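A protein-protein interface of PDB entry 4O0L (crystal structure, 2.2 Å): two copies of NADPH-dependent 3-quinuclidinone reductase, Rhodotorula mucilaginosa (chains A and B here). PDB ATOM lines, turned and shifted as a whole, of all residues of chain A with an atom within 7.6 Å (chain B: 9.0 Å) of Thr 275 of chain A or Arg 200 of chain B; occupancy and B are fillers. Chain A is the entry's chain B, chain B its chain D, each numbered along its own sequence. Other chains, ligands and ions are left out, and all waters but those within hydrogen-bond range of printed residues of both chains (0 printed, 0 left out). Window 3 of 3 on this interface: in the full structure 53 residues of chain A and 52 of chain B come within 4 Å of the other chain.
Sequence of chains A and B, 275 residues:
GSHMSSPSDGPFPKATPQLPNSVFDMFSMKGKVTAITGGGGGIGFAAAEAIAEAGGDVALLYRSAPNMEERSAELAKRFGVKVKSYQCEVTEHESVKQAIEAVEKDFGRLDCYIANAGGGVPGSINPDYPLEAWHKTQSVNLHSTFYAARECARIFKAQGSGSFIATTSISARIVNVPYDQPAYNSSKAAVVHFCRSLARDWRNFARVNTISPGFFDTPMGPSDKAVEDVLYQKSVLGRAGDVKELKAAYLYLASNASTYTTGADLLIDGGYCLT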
ATOM      1  N   ILE A 174       5.321  -7.711  12.716  1.00  0.00           N
ATOM      2  CA  ILE A 174       5.528  -8.545  11.533  1.00  0.00           C
ATOM      3  C   ILE A 174       6.557  -7.942  10.558  1.00  0.00           C
ATOM      4  O   ILE A 174       6.944  -6.792  10.680  1.00  0.00           O
ATOM      5  CB  ILE A 174       4.185  -8.904  10.793  1.00  0.00           C
ATOM      6  CG1 ILE A 174       3.408  -7.651  10.381  1.00  0.00           C
ATOM      7  CG2 ILE A 174       3.336  -9.893  11.617  1.00  0.00           C
ATOM      8  CD1 ILE A 174       4.015  -6.955   9.191  1.00  0.00           C
ATOM      9  N   GLN A 233      -4.720 -10.052   0.521  1.00  0.00           N
ATOM     10  CA  GLN A 233      -4.711 -11.450   0.979  1.00  0.00           C
ATOM     11  C   GLN A 233      -4.388 -11.640   2.470  1.00  0.00           C
ATOM     12  O   GLN A 233      -4.793 -12.630   3.051  1.00  0.00           O
ATOM     13  CB  GLN A 233      -3.846 -12.349   0.075  1.00  0.00           C
ATOM     14  CG  GLN A 233      -2.357 -12.068   0.052  1.00  0.00           C
ATOM     15  CD  GLN A 233      -1.630 -12.785  -1.117  1.00  0.00           C
ATOM     16  OE1 GLN A 233      -1.840 -13.973  -1.362  1.00  0.00           O
ATOM     17  NE2 GLN A 233      -0.754 -12.054  -1.820  1.00  0.00           N
ATOM     18  N   LYS A 234      -3.719 -10.678   3.088  1.00  0.00           N
ATOM     19  CA  LYS A 234      -3.322 -10.788   4.508  1.00  0.00           C
ATOM     20  C   LYS A 234      -4.355 -10.190   5.484  1.00  0.00           C
ATOM     21  O   LYS A 234      -4.714 -10.814   6.482  1.00  0.00           O
ATOM     22  CB  LYS A 234      -1.943 -10.160   4.747  1.00  0.00           C
ATOM     23  CG  LYS A 234      -0.774 -10.952   4.197  1.00  0.00           C
ATOM     24  CD  LYS A 234      -0.260 -11.952   5.194  1.00  0.00           C
ATOM     25  CE  LYS A 234       0.292 -11.252   6.424  1.00  0.00           C
ATOM     26  NZ  LYS A 234       0.083 -11.985   7.701  1.00  0.00           N
ATOM     27  N   SER A 235      -4.829  -8.988   5.216  1.00  0.00           N
ATOM     28  CA  SER A 235      -5.893  -8.456   6.067  1.00  0.00           C
ATOM     29  C   SER A 235      -7.187  -9.191   5.723  1.00  0.00           C
ATOM     30  O   SER A 235      -7.569  -9.288   4.555  1.00  0.00           O
ATOM     31  CB  SER A 235      -6.038  -6.940   5.940  1.00  0.00           C
ATOM     32  OG  SER A 235      -6.997  -6.578   4.980  1.00  0.00           O
ATOM     33  N   VAL A 236      -7.842  -9.722   6.749  1.00  0.00           N
ATOM     34  CA  VAL A 236      -9.052 -10.525   6.585  1.00  0.00           C
ATOM     35  C   VAL A 236     -10.249  -9.686   6.081  1.00  0.00           C
ATOM     36  O   VAL A 236     -11.212 -10.222   5.561  1.00  0.00           O
ATOM     37  CB  VAL A 236      -9.404 -11.306   7.894  1.00  0.00           C
ATOM     38  CG1 VAL A 236      -8.199 -12.126   8.373  1.00  0.00           C
ATOM     39  CG2 VAL A 236      -9.870 -10.376   9.020  1.00  0.00           C
ATOM     40  N   LEU A 237     -10.166  -8.374   6.250  1.00  0.00           N
ATOM     41  CA  LEU A 237     -11.191  -7.451   5.759  1.00  0.00           C
ATOM     42  C   LEU A 237     -10.948  -6.994   4.310  1.00  0.00           C
ATOM     43  O   LEU A 237     -11.738  -6.254   3.780  1.00  0.00           O
ATOM     44  CB  LEU A 237     -11.347  -6.236   6.697  1.00  0.00           C
ATOM     45  CG  LEU A 237     -11.615  -6.438   8.204  1.00  0.00           C
ATOM     46  CD1 LEU A 237     -11.666  -5.096   8.951  1.00  0.00           C
ATOM     47  CD2 LEU A 237     -12.906  -7.182   8.446  1.00  0.00           C
ATOM     48  N   GLY A 271      -6.852  -7.345  10.785  1.00  0.00           N
ATOM     49  CA  GLY A 271      -6.493  -8.757  10.889  1.00  0.00           C
ATOM     50  C   GLY A 271      -5.264  -9.150  10.107  1.00  0.00           C
ATOM     51  O   GLY A 271      -5.007 -10.330   9.953  1.00  0.00           O
ATOM     52  N   TYR A 272      -4.504  -8.172   9.634  1.00  0.00           N
ATOM     53  CA  TYR A 272      -3.276  -8.411   8.853  1.00  0.00           C
ATOM     54  C   TYR A 272      -2.327  -9.402   9.531  1.00  0.00           C
ATOM     55  O   TYR A 272      -1.745 -10.250   8.873  1.00  0.00           O
ATOM     56  CB  TYR A 272      -2.521  -7.079   8.594  1.00  0.00           C
ATOM     57  CG  TYR A 272      -1.319  -7.209   7.659  1.00  0.00           C
ATOM     58  CD1 TYR A 272      -0.070  -7.709   8.130  1.00  0.00           C
ATOM     59  CD2 TYR A 272      -1.399  -6.854   6.322  1.00  0.00           C
ATOM     60  CE1 TYR A 272       1.028  -7.832   7.280  1.00  0.00           C
ATOM     61  CE2 TYR A 272      -0.300  -6.961   5.467  1.00  0.00           C
ATOM     62  CZ  TYR A 272       0.911  -7.457   5.946  1.00  0.00           C
ATOM     63  OH  TYR A 272       2.007  -7.565   5.069  1.00  0.00           O
ATOM     64  N   CYS A 273      -2.176  -9.271  10.845  1.00  0.00           N
ATOM     65  CA  CYS A 273      -1.212 -10.091  11.600  1.00  0.00           C
ATOM     66  C   CYS A 273      -1.730 -11.484  12.005  1.00  0.00           C
ATOM     67  O   CYS A 273      -1.023 -12.233  12.670  1.00  0.00           O
ATOM     68  CB  CYS A 273      -0.771  -9.319  12.865  1.00  0.00           C
ATOM     69  SG  CYS A 273       0.185  -7.847  12.481  1.00  0.00           S
ATOM     70  N   LEU A 274      -2.958 -11.826  11.619  1.00  0.00           N
ATOM     71  CA  LEU A 274      -3.573 -13.058  12.095  1.00  0.00           C
ATOM     72  C   LEU A 274      -2.964 -14.313  11.447  1.00  0.00           C
ATOM     73  O   LEU A 274      -2.708 -15.312  12.133  1.00  0.00           O
ATOM     74  CB  LEU A 274      -5.070 -13.039  11.875  1.00  0.00           C
ATOM     75  CG  LEU A 274      -5.873 -12.081  12.760  1.00  0.00           C
ATOM     76  CD1 LEU A 274      -7.292 -12.001  12.216  1.00  0.00           C
ATOM     77  CD2 LEU A 274      -5.846 -12.556  14.194  1.00  0.00           C
ATOM     78  N   THR A 275      -2.705 -14.221  10.146  1.00  0.00           N
ATOM     79  CA  THR A 275      -2.266 -15.364   9.372  1.00  0.00           C
ATOM     80  C   THR A 275      -0.766 -15.372   9.105  1.00  0.00           C
ATOM     81  O   THR A 275      -0.102 -14.295   9.097  1.00  0.00           O
ATOM     82  CB  THR A 275      -3.033 -15.451   8.038  1.00  0.00           C
ATOM     83  OG1 THR A 275      -2.630 -14.387   7.195  1.00  0.00           O
ATOM     84  CG2 THR A 275      -4.542 -15.387   8.281  1.00  0.00           C
ATOM     85  OXT THR A 275      -0.200 -16.476   8.907  1.00  0.00           O
ATOM     86  N   HIS B 193      -6.774 -17.101  21.373  1.00  0.00           N
ATOM     87  CA  HIS B 193      -6.417 -17.535  20.034  1.00  0.00           C
ATOM     88  C   HIS B 193      -7.598 -18.150  19.284  1.00  0.00           C
ATOM     89  O   HIS B 193      -7.629 -18.152  18.046  1.00  0.00           O
ATOM     90  CB  HIS B 193      -5.205 -18.485  20.079  1.00  0.00           C
ATOM     91  CG  HIS B 193      -4.503 -18.619  18.758  1.00  0.00           C
ATOM     92  ND1 HIS B 193      -4.055 -17.544  18.047  1.00  0.00           N
ATOM     93  CD2 HIS B 193      -4.177 -19.709  18.027  1.00  0.00           C
ATOM     94  CE1 HIS B 193      -3.476 -17.956  16.930  1.00  0.00           C
ATOM     95  NE2 HIS B 193      -3.529 -19.270  16.904  1.00  0.00           N
ATOM     96  N   PHE B 194      -8.577 -18.670  20.026  1.00  0.00           N
ATOM     97  CA  PHE B 194      -9.831 -19.090  19.451  1.00  0.00           C
ATOM     98  C   PHE B 194     -10.470 -17.866  18.788  1.00  0.00           C
ATOM     99  O   PHE B 194     -10.918 -17.937  17.648  1.00  0.00           O
ATOM    100  CB  PHE B 194     -10.770 -19.670  20.508  1.00  0.00           C
ATOM    101  CG  PHE B 194     -12.147 -20.012  19.999  1.00  0.00           C
ATOM    102  CD1 PHE B 194     -12.340 -20.933  18.960  1.00  0.00           C
ATOM    103  CD2 PHE B 194     -13.285 -19.416  20.559  1.00  0.00           C
ATOM    104  CE1 PHE B 194     -13.624 -21.246  18.494  1.00  0.00           C
ATOM    105  CE2 PHE B 194     -14.563 -19.727  20.083  1.00  0.00           C
ATOM    106  CZ  PHE B 194     -14.720 -20.648  19.057  1.00  0.00           C
ATOM    107  N   CYS B 195     -10.501 -16.744  19.506  1.00  0.00           N
ATOM    108  CA  CYS B 195     -11.104 -15.536  18.970  1.00  0.00           C
ATOM    109  C   CYS B 195     -10.329 -15.028  17.762  1.00  0.00           C
ATOM    110  O   CYS B 195     -10.927 -14.584  16.794  1.00  0.00           O
ATOM    111  CB  CYS B 195     -11.266 -14.464  20.053  1.00  0.00           C
ATOM    112  SG  CYS B 195     -12.576 -14.877  21.240  1.00  0.00           S
ATOM    113  N   ARG B 196      -8.998 -15.111  17.818  1.00  0.00           N
ATOM    114  CA  ARG B 196      -8.179 -14.708  16.661  1.00  0.00           C
ATOM    115  C   ARG B 196      -8.540 -15.562  15.428  1.00  0.00           C
ATOM    116  O   ARG B 196      -8.665 -15.045  14.325  1.00  0.00           O
ATOM    117  CB  ARG B 196      -6.680 -14.792  16.953  1.00  0.00           C
ATOM    118  CG  ARG B 196      -6.163 -13.667  17.842  1.00  0.00           C
ATOM    119  CD  ARG B 196      -4.634 -13.545  17.799  1.00  0.00           C
ATOM    120  NE  ARG B 196      -3.972 -14.555  18.614  1.00  0.00           N
ATOM    121  CZ  ARG B 196      -3.319 -14.318  19.755  1.00  0.00           C
ATOM    122  NH1 ARG B 196      -3.248 -13.101  20.250  1.00  0.00           N
ATOM    123  NH2 ARG B 196      -2.742 -15.322  20.414  1.00  0.00           N
ATOM    124  N   SER B 197      -8.747 -16.861  15.652  1.00  0.00           N
ATOM    125  CA  SER B 197      -9.091 -17.796  14.560  1.00  0.00           C
ATOM    126  C   SER B 197     -10.482 -17.487  13.989  1.00  0.00           C
ATOM    127  O   SER B 197     -10.698 -17.571  12.775  1.00  0.00           O
ATOM    128  CB  SER B 197      -8.983 -19.229  15.040  1.00  0.00           C
ATOM    129  OG  SER B 197      -7.633 -19.500  15.492  1.00  0.00           O
ATOM    130  N   LEU B 198     -11.400 -17.086  14.870  1.00  0.00           N
ATOM    131  CA  LEU B 198     -12.745 -16.674  14.477  1.00  0.00           C
ATOM    132  C   LEU B 198     -12.736 -15.401  13.658  1.00  0.00           C
ATOM    133  O   LEU B 198     -13.535 -15.269  12.733  1.00  0.00           O
ATOM    134  CB  LEU B 198     -13.621 -16.409  15.712  1.00  0.00           C
ATOM    135  CG  LEU B 198     -14.193 -17.539  16.546  1.00  0.00           C
ATOM    136  CD1 LEU B 198     -15.147 -16.934  17.573  1.00  0.00           C
ATOM    137  CD2 LEU B 198     -14.882 -18.573  15.686  1.00  0.00           C
ATOM    138  N   ALA B 199     -11.849 -14.470  14.023  1.00  0.00           N
ATOM    139  CA  ALA B 199     -11.699 -13.203  13.324  1.00  0.00           C
ATOM    140  C   ALA B 199     -11.402 -13.442  11.847  1.00  0.00           C
ATOM    141  O   ALA B 199     -11.934 -12.737  10.980  1.00  0.00           O
ATOM    142  CB  ALA B 199     -10.613 -12.361  13.961  1.00  0.00           C
ATOM    143  N   ARG B 200     -10.566 -14.438  11.555  1.00  0.00           N
ATOM    144  CA  ARG B 200     -10.282 -14.812  10.165  1.00  0.00           C
ATOM    145  C   ARG B 200     -11.486 -15.573   9.583  1.00  0.00           C
ATOM    146  O   ARG B 200     -11.994 -15.216   8.516  1.00  0.00           O
ATOM    147  CB  ARG B 200      -9.005 -15.613  10.055  1.00  0.00           C
ATOM    148  CG  ARG B 200      -8.498 -15.822   8.604  1.00  0.00           C
ATOM    149  CD  ARG B 200      -9.193 -16.990   7.904  1.00  0.00           C
ATOM    150  NE  ARG B 200      -8.878 -17.016   6.472  1.00  0.00           N
ATOM    151  CZ  ARG B 200      -9.256 -17.955   5.613  1.00  0.00           C
ATOM    152  NH1 ARG B 200      -9.939 -19.018   6.014  1.00  0.00           N
ATOM    153  NH2 ARG B 200      -8.910 -17.847   4.358  1.00  0.00           N
ATOM    154  N   ASP B 201     -11.962 -16.583  10.326  1.00  0.00           N
ATOM    155  CA  ASP B 201     -13.100 -17.405   9.937  1.00  0.00           C
ATOM    156  C   ASP B 201     -14.322 -16.575   9.518  1.00  0.00           C
ATOM    157  O   ASP B 201     -14.943 -16.799   8.463  1.00  0.00           O
ATOM    158  CB  ASP B 201     -13.429 -18.335  11.092  1.00  0.00           C
ATOM    159  CG  ASP B 201     -14.318 -19.518  10.666  1.00  0.00           C
ATOM    160  OD1 ASP B 201     -14.369 -19.852   9.442  1.00  0.00           O
ATOM    161  OD2 ASP B 201     -14.956 -20.119  11.559  1.00  0.00           O
ATOM    162  N   TRP B 202     -14.641 -15.580  10.348  1.00  0.00           N
ATOM    163  CA  TRP B 202     -15.854 -14.794  10.211  1.00  0.00           C
ATOM    164  C   TRP B 202     -15.649 -13.488   9.457  1.00  0.00           C
ATOM    165  O   TRP B 202     -16.514 -12.607   9.494  1.00  0.00           O
ATOM    166  CB  TRP B 202     -16.365 -14.469  11.608  1.00  0.00           C
ATOM    167  CG  TRP B 202     -16.951 -15.626  12.318  1.00  0.00           C
ATOM    168  CD1 TRP B 202     -16.993 -16.930  11.897  1.00  0.00           C
ATOM    169  CD2 TRP B 202     -17.549 -15.600  13.613  1.00  0.00           C
ATOM    170  NE1 TRP B 202     -17.585 -17.706  12.856  1.00  0.00           N
ATOM    171  CE2 TRP B 202     -17.937 -16.916  13.919  1.00  0.00           C
ATOM    172  CE3 TRP B 202     -17.758 -14.589  14.566  1.00  0.00           C
ATOM    173  CZ2 TRP B 202     -18.562 -17.252  15.128  1.00  0.00           C
ATOM    174  CZ3 TRP B 202     -18.369 -14.910  15.757  1.00  0.00           C
ATOM    175  CH2 TRP B 202     -18.778 -16.235  16.027  1.00  0.00           C
ATOM    176  N   ARG B 203     -14.515 -13.368   8.785  1.00  0.00           N
ATOM    177  CA  ARG B 203     -14.053 -12.096   8.181  1.00  0.00           C
ATOM    178  C   ARG B 203     -15.065 -11.394   7.266  1.00  0.00           C
ATOM    179  O   ARG B 203     -15.022 -10.182   7.127  1.00  0.00           O
ATOM    180  CB  ARG B 203     -12.760 -12.318   7.431  1.00  0.00           C
ATOM    181  CG  ARG B 203     -12.886 -13.224   6.246  1.00  0.00           C
ATOM    182  CD  ARG B 203     -11.549 -13.642   5.650  1.00  0.00           C
ATOM    183  NE  ARG B 203     -11.772 -14.567   4.533  1.00  0.00           N
ATOM    184  CZ  ARG B 203     -12.111 -15.840   4.664  1.00  0.00           C
ATOM    185  NH1 ARG B 203     -12.335 -16.578   3.581  1.00  0.00           N
ATOM    186  NH2 ARG B 203     -12.205 -16.382   5.875  1.00  0.00           N
ATOM    187  N   ASN B 204     -15.967 -12.157   6.662  1.00  0.00           N
ATOM    188  CA  ASN B 204     -16.932 -11.567   5.716  1.00  0.00           C
ATOM    189  C   ASN B 204     -18.166 -11.015   6.400  1.00  0.00           C
ATOM    190  O   ASN B 204     -18.956 -10.344   5.755  1.00  0.00           O
ATOM    191  CB  ASN B 204     -17.356 -12.575   4.633  1.00  0.00           C
ATOM    192  CG  ASN B 204     -16.249 -12.888   3.651  1.00  0.00           C
ATOM    193  OD1 ASN B 204     -16.037 -14.038   3.314  1.00  0.00           O
ATOM    194  ND2 ASN B 204     -15.536 -11.898   3.209  1.00  0.00           N
ATOM    195  N   PHE B 205     -18.334 -11.307   7.697  1.00  0.00           N
ATOM    196  CA  PHE B 205     -19.573 -10.894   8.359  1.00  0.00           C
ATOM    197  C   PHE B 205     -19.441 -10.412   9.788  1.00  0.00           C
ATOM    198  O   PHE B 205     -20.427 -10.011  10.389  1.00  0.00           O
ATOM    199  CB  PHE B 205     -20.651 -11.986   8.245  1.00  0.00           C
ATOM    200  CG  PHE B 205     -20.206 -13.347   8.705  1.00  0.00           C
ATOM    201  CD1 PHE B 205     -20.195 -13.678  10.067  1.00  0.00           C
ATOM    202  CD2 PHE B 205     -19.793 -14.310   7.769  1.00  0.00           C
ATOM    203  CE1 PHE B 205     -19.786 -14.931  10.493  1.00  0.00           C
ATOM    204  CE2 PHE B 205     -19.372 -15.584   8.186  1.00  0.00           C
ATOM    205  CZ  PHE B 205     -19.363 -15.899   9.547  1.00  0.00           C
ATOM    206  N   ALA B 206     -18.238 -10.446  10.352  1.00  0.00           N
ATOM    207  CA  ALA B 206     -18.102 -10.021  11.747  1.00  0.00           C
ATOM    208  C   ALA B 206     -16.687  -9.701  12.134  1.00  0.00           C
ATOM    209  O   ALA B 206     -15.743 -10.115  11.459  1.00  0.00           O
ATOM    210  CB  ALA B 206     -18.686 -11.080  12.696  1.00  0.00           C
ATOM    211  N   ARG B 207     -16.563  -8.955  13.231  1.00  0.00           N
ATOM    212  CA  ARG B 207     -15.297  -8.716  13.873  1.00  0.00           C
ATOM    213  C   ARG B 207     -15.269  -9.459  15.213  1.00  0.00           C
ATOM    214  O   ARG B 207     -16.317  -9.653  15.839  1.00  0.00           O
ATOM    215  CB  ARG B 207     -15.067  -7.235  14.076  1.00  0.00           C
ATOM    216  CG  ARG B 207     -14.878  -6.423  12.803  1.00  0.00           C
ATOM    217  CD  ARG B 207     -14.609  -4.963  13.134  1.00  0.00           C
ATOM    218  NE  ARG B 207     -15.718  -4.346  13.847  1.00  0.00           N
ATOM    219  CZ  ARG B 207     -15.745  -4.039  15.134  1.00  0.00           C
ATOM    220  NH1 ARG B 207     -14.681  -4.298  15.916  1.00  0.00           N
ATOM    221  NH2 ARG B 207     -16.835  -3.474  15.656  1.00  0.00           N
ATOM    222  N   VAL B 208     -14.071  -9.884  15.623  1.00  0.00           N
ATOM    223  CA  VAL B 208     -13.870 -10.661  16.846  1.00  0.00           C
ATOM    224  C   VAL B 208     -12.620 -10.152  17.557  1.00  0.00           C
ATOM    225  O   VAL B 208     -11.540 -10.063  16.952  1.00  0.00           O
ATOM    226  CB  VAL B 208     -13.707 -12.193  16.562  1.00  0.00           C
ATOM    227  CG1 VAL B 208     -13.732 -13.000  17.879  1.00  0.00           C
ATOM    228  CG2 VAL B 208     -14.786 -12.701  15.600  1.00  0.00           C
ATOM    229  N   ASN B 209     -12.778  -9.785  18.833  1.00  0.00           N
ATOM    230  CA  ASN B 209     -11.667  -9.257  19.650  1.00  0.00           C
ATOM    231  C   ASN B 209     -11.815  -9.711  21.087  1.00  0.00           C
ATOM    232  O   ASN B 209     -12.881 -10.154  21.484  1.00  0.00           O
ATOM    233  CB  ASN B 209     -11.612  -7.735  19.597  1.00  0.00           C
ATOM    234  CG  ASN B 209     -11.537  -7.209  18.185  1.00  0.00           C
ATOM    235  OD1 ASN B 209     -12.559  -6.900  17.571  1.00  0.00           O
ATOM    236  ND2 ASN B 209     -10.333  -7.133  17.648  1.00  0.00           N
ATOM    237  N   THR B 262      -9.917  -6.077  14.355  1.00  0.00           N
ATOM    238  CA  THR B 262     -10.343  -7.470  14.483  1.00  0.00           C
ATOM    239  C   THR B 262      -9.123  -8.377  14.736  1.00  0.00           C
ATOM    240  O   THR B 262      -8.031  -8.118  14.208  1.00  0.00           O
ATOM    241  CB  THR B 262     -11.194  -7.921  13.274  1.00  0.00           C
ATOM    242  OG1 THR B 262     -11.906  -9.129  13.599  1.00  0.00           O
ATOM    243  CG2 THR B 262     -10.338  -8.115  12.015  1.00  0.00           C
ATOM    244  N   GLY B 263      -9.304  -9.396  15.568  1.00  0.00           N
ATOM    245  CA  GLY B 263      -8.199 -10.273  15.962  1.00  0.00           C
ATOM    246  C   GLY B 263      -7.316  -9.701  17.062  1.00  0.00           C
ATOM    247  O   GLY B 263      -6.244 -10.259  17.382  1.00  0.00           O
ATOM    248  N   ALA B 264      -7.768  -8.601  17.664  1.00  0.00           N
ATOM    249  CA  ALA B 264      -6.986  -7.888  18.669  1.00  0.00           C
ATOM    250  C   ALA B 264      -7.301  -8.307  20.095  1.00  0.00           C
ATOM    251  O   ALA B 264      -8.401  -8.758  20.398  1.00  0.00           O
ATOM    252  CB  ALA B 264      -7.120  -6.391  18.494  1.00  0.00           C
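Printed residues of chain B within 4 Å of Thr 275 of chain A: Arg 200 (3.99 Å).
Of the printed residues of chain A, Arg 200 of chain B touches Val 236 (3.7 Å) and Thr 275 (3.99 Å).
Ala 199 of chain B touches two residues of chain A.
Of the printed residues of chain A, Arg 196 of chain B touches Leu 274 (3.6 Å).
Printed residues of chain B within 4 Å of Leu 237 of chain A: Arg 203 (3.9 Å).
Printed residues of chain A within 4 Å of Thr 262 of chain B: Val 236 (3.8 Å) and Gly 271 (3.7 Å).
Arg 207 of chain B touches none of the printed residues of chain A.
Ser 197 of chain B touches none of the printed residues of chain A.
The nearest printed residue of chain A that does not touch Arg 200 of chain B is Leu 274 of chain A (4.1 Å).
The nearest printed residue of chain A that does not touch Arg 203 of chain B is Ser 235 of chain A (6.0 Å).
The chain-end carboxylate of Thr 275 of chain A is in salt-bridge range of the side-chain amino group of Lys 234 of chain A, 2.7 Å away.
NE of Arg 196 of chain B sits at hydrogen-bond distance from ND1 of His 193 of chain B (3.0 Å).
The backbone NH of Val 208 of chain B sits at hydrogen-bond distance from the side-chain hydroxyl of Thr 262 of chain B (3.1 Å).
The backbone NH of Gly 263 of chain B lies within hydrogen-bond range of the backbone carbonyl oxygen of Val 208 of chain B (2.7 Å).
The side-chain amide nitrogen (ND2) of Asn 209 of chain B lies close to the backbone NH (N) of Thr 262 of chain B (3.5 Å).
The side-chain amide nitrogen of Asn 209 of chain B sits close to the backbone NH of Gly 263 of chain B (3.2 Å).
Of the 20 printed residues of chain B, 6 touch a printed residue of chain A.
Of the 11 printed residues of chain A, 5 touch a printed residue of chain B.
Printed residues of chain A that touch a printed residue of chain B: Val 236, Leu 237, Gly 271, Leu 274 and Thr 275.
Hydrophobic or aromatic side chains of chain A that line the printed part of chain B: Val 236, Leu 237 and Leu 274.
Among the printed residues, no Asp or Glu carboxylate lies within 4 Å of a Lys or Arg side-chain nitrogen of the other chain.
Among the printed residues, merely in contact across the chains: Val 236 of chain A with Ala 199 of chain B (3.7 Å), Val 236 of chain A with Arg 200 of chain B (3.7 Å), Val 236 of chain A with Arg 203 of chain B (3.2 Å), Val 236 of chain A with Thr 262 of chain B (3.8 Å), Leu 237 of chain A with Arg 203 of chain B (3.9 Å), Gly 271 of chain A with Thr 262 of chain B (3.7 Å), Leu 274 of chain A with Arg 196 of chain B (3.6 Å), Leu 274 of chain A with Ala 199 of chain B (3.8 Å), Leu 274 of chain A with Gly 263 of chain B (3.7 Å) and Thr 275 of chain A with Arg 200 of chain B (3.99 Å).
No position is printed for both chains.
Of the 10 pairs that touch across the chains among the printed residues, none has its exchanged pair printed and touching as well.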
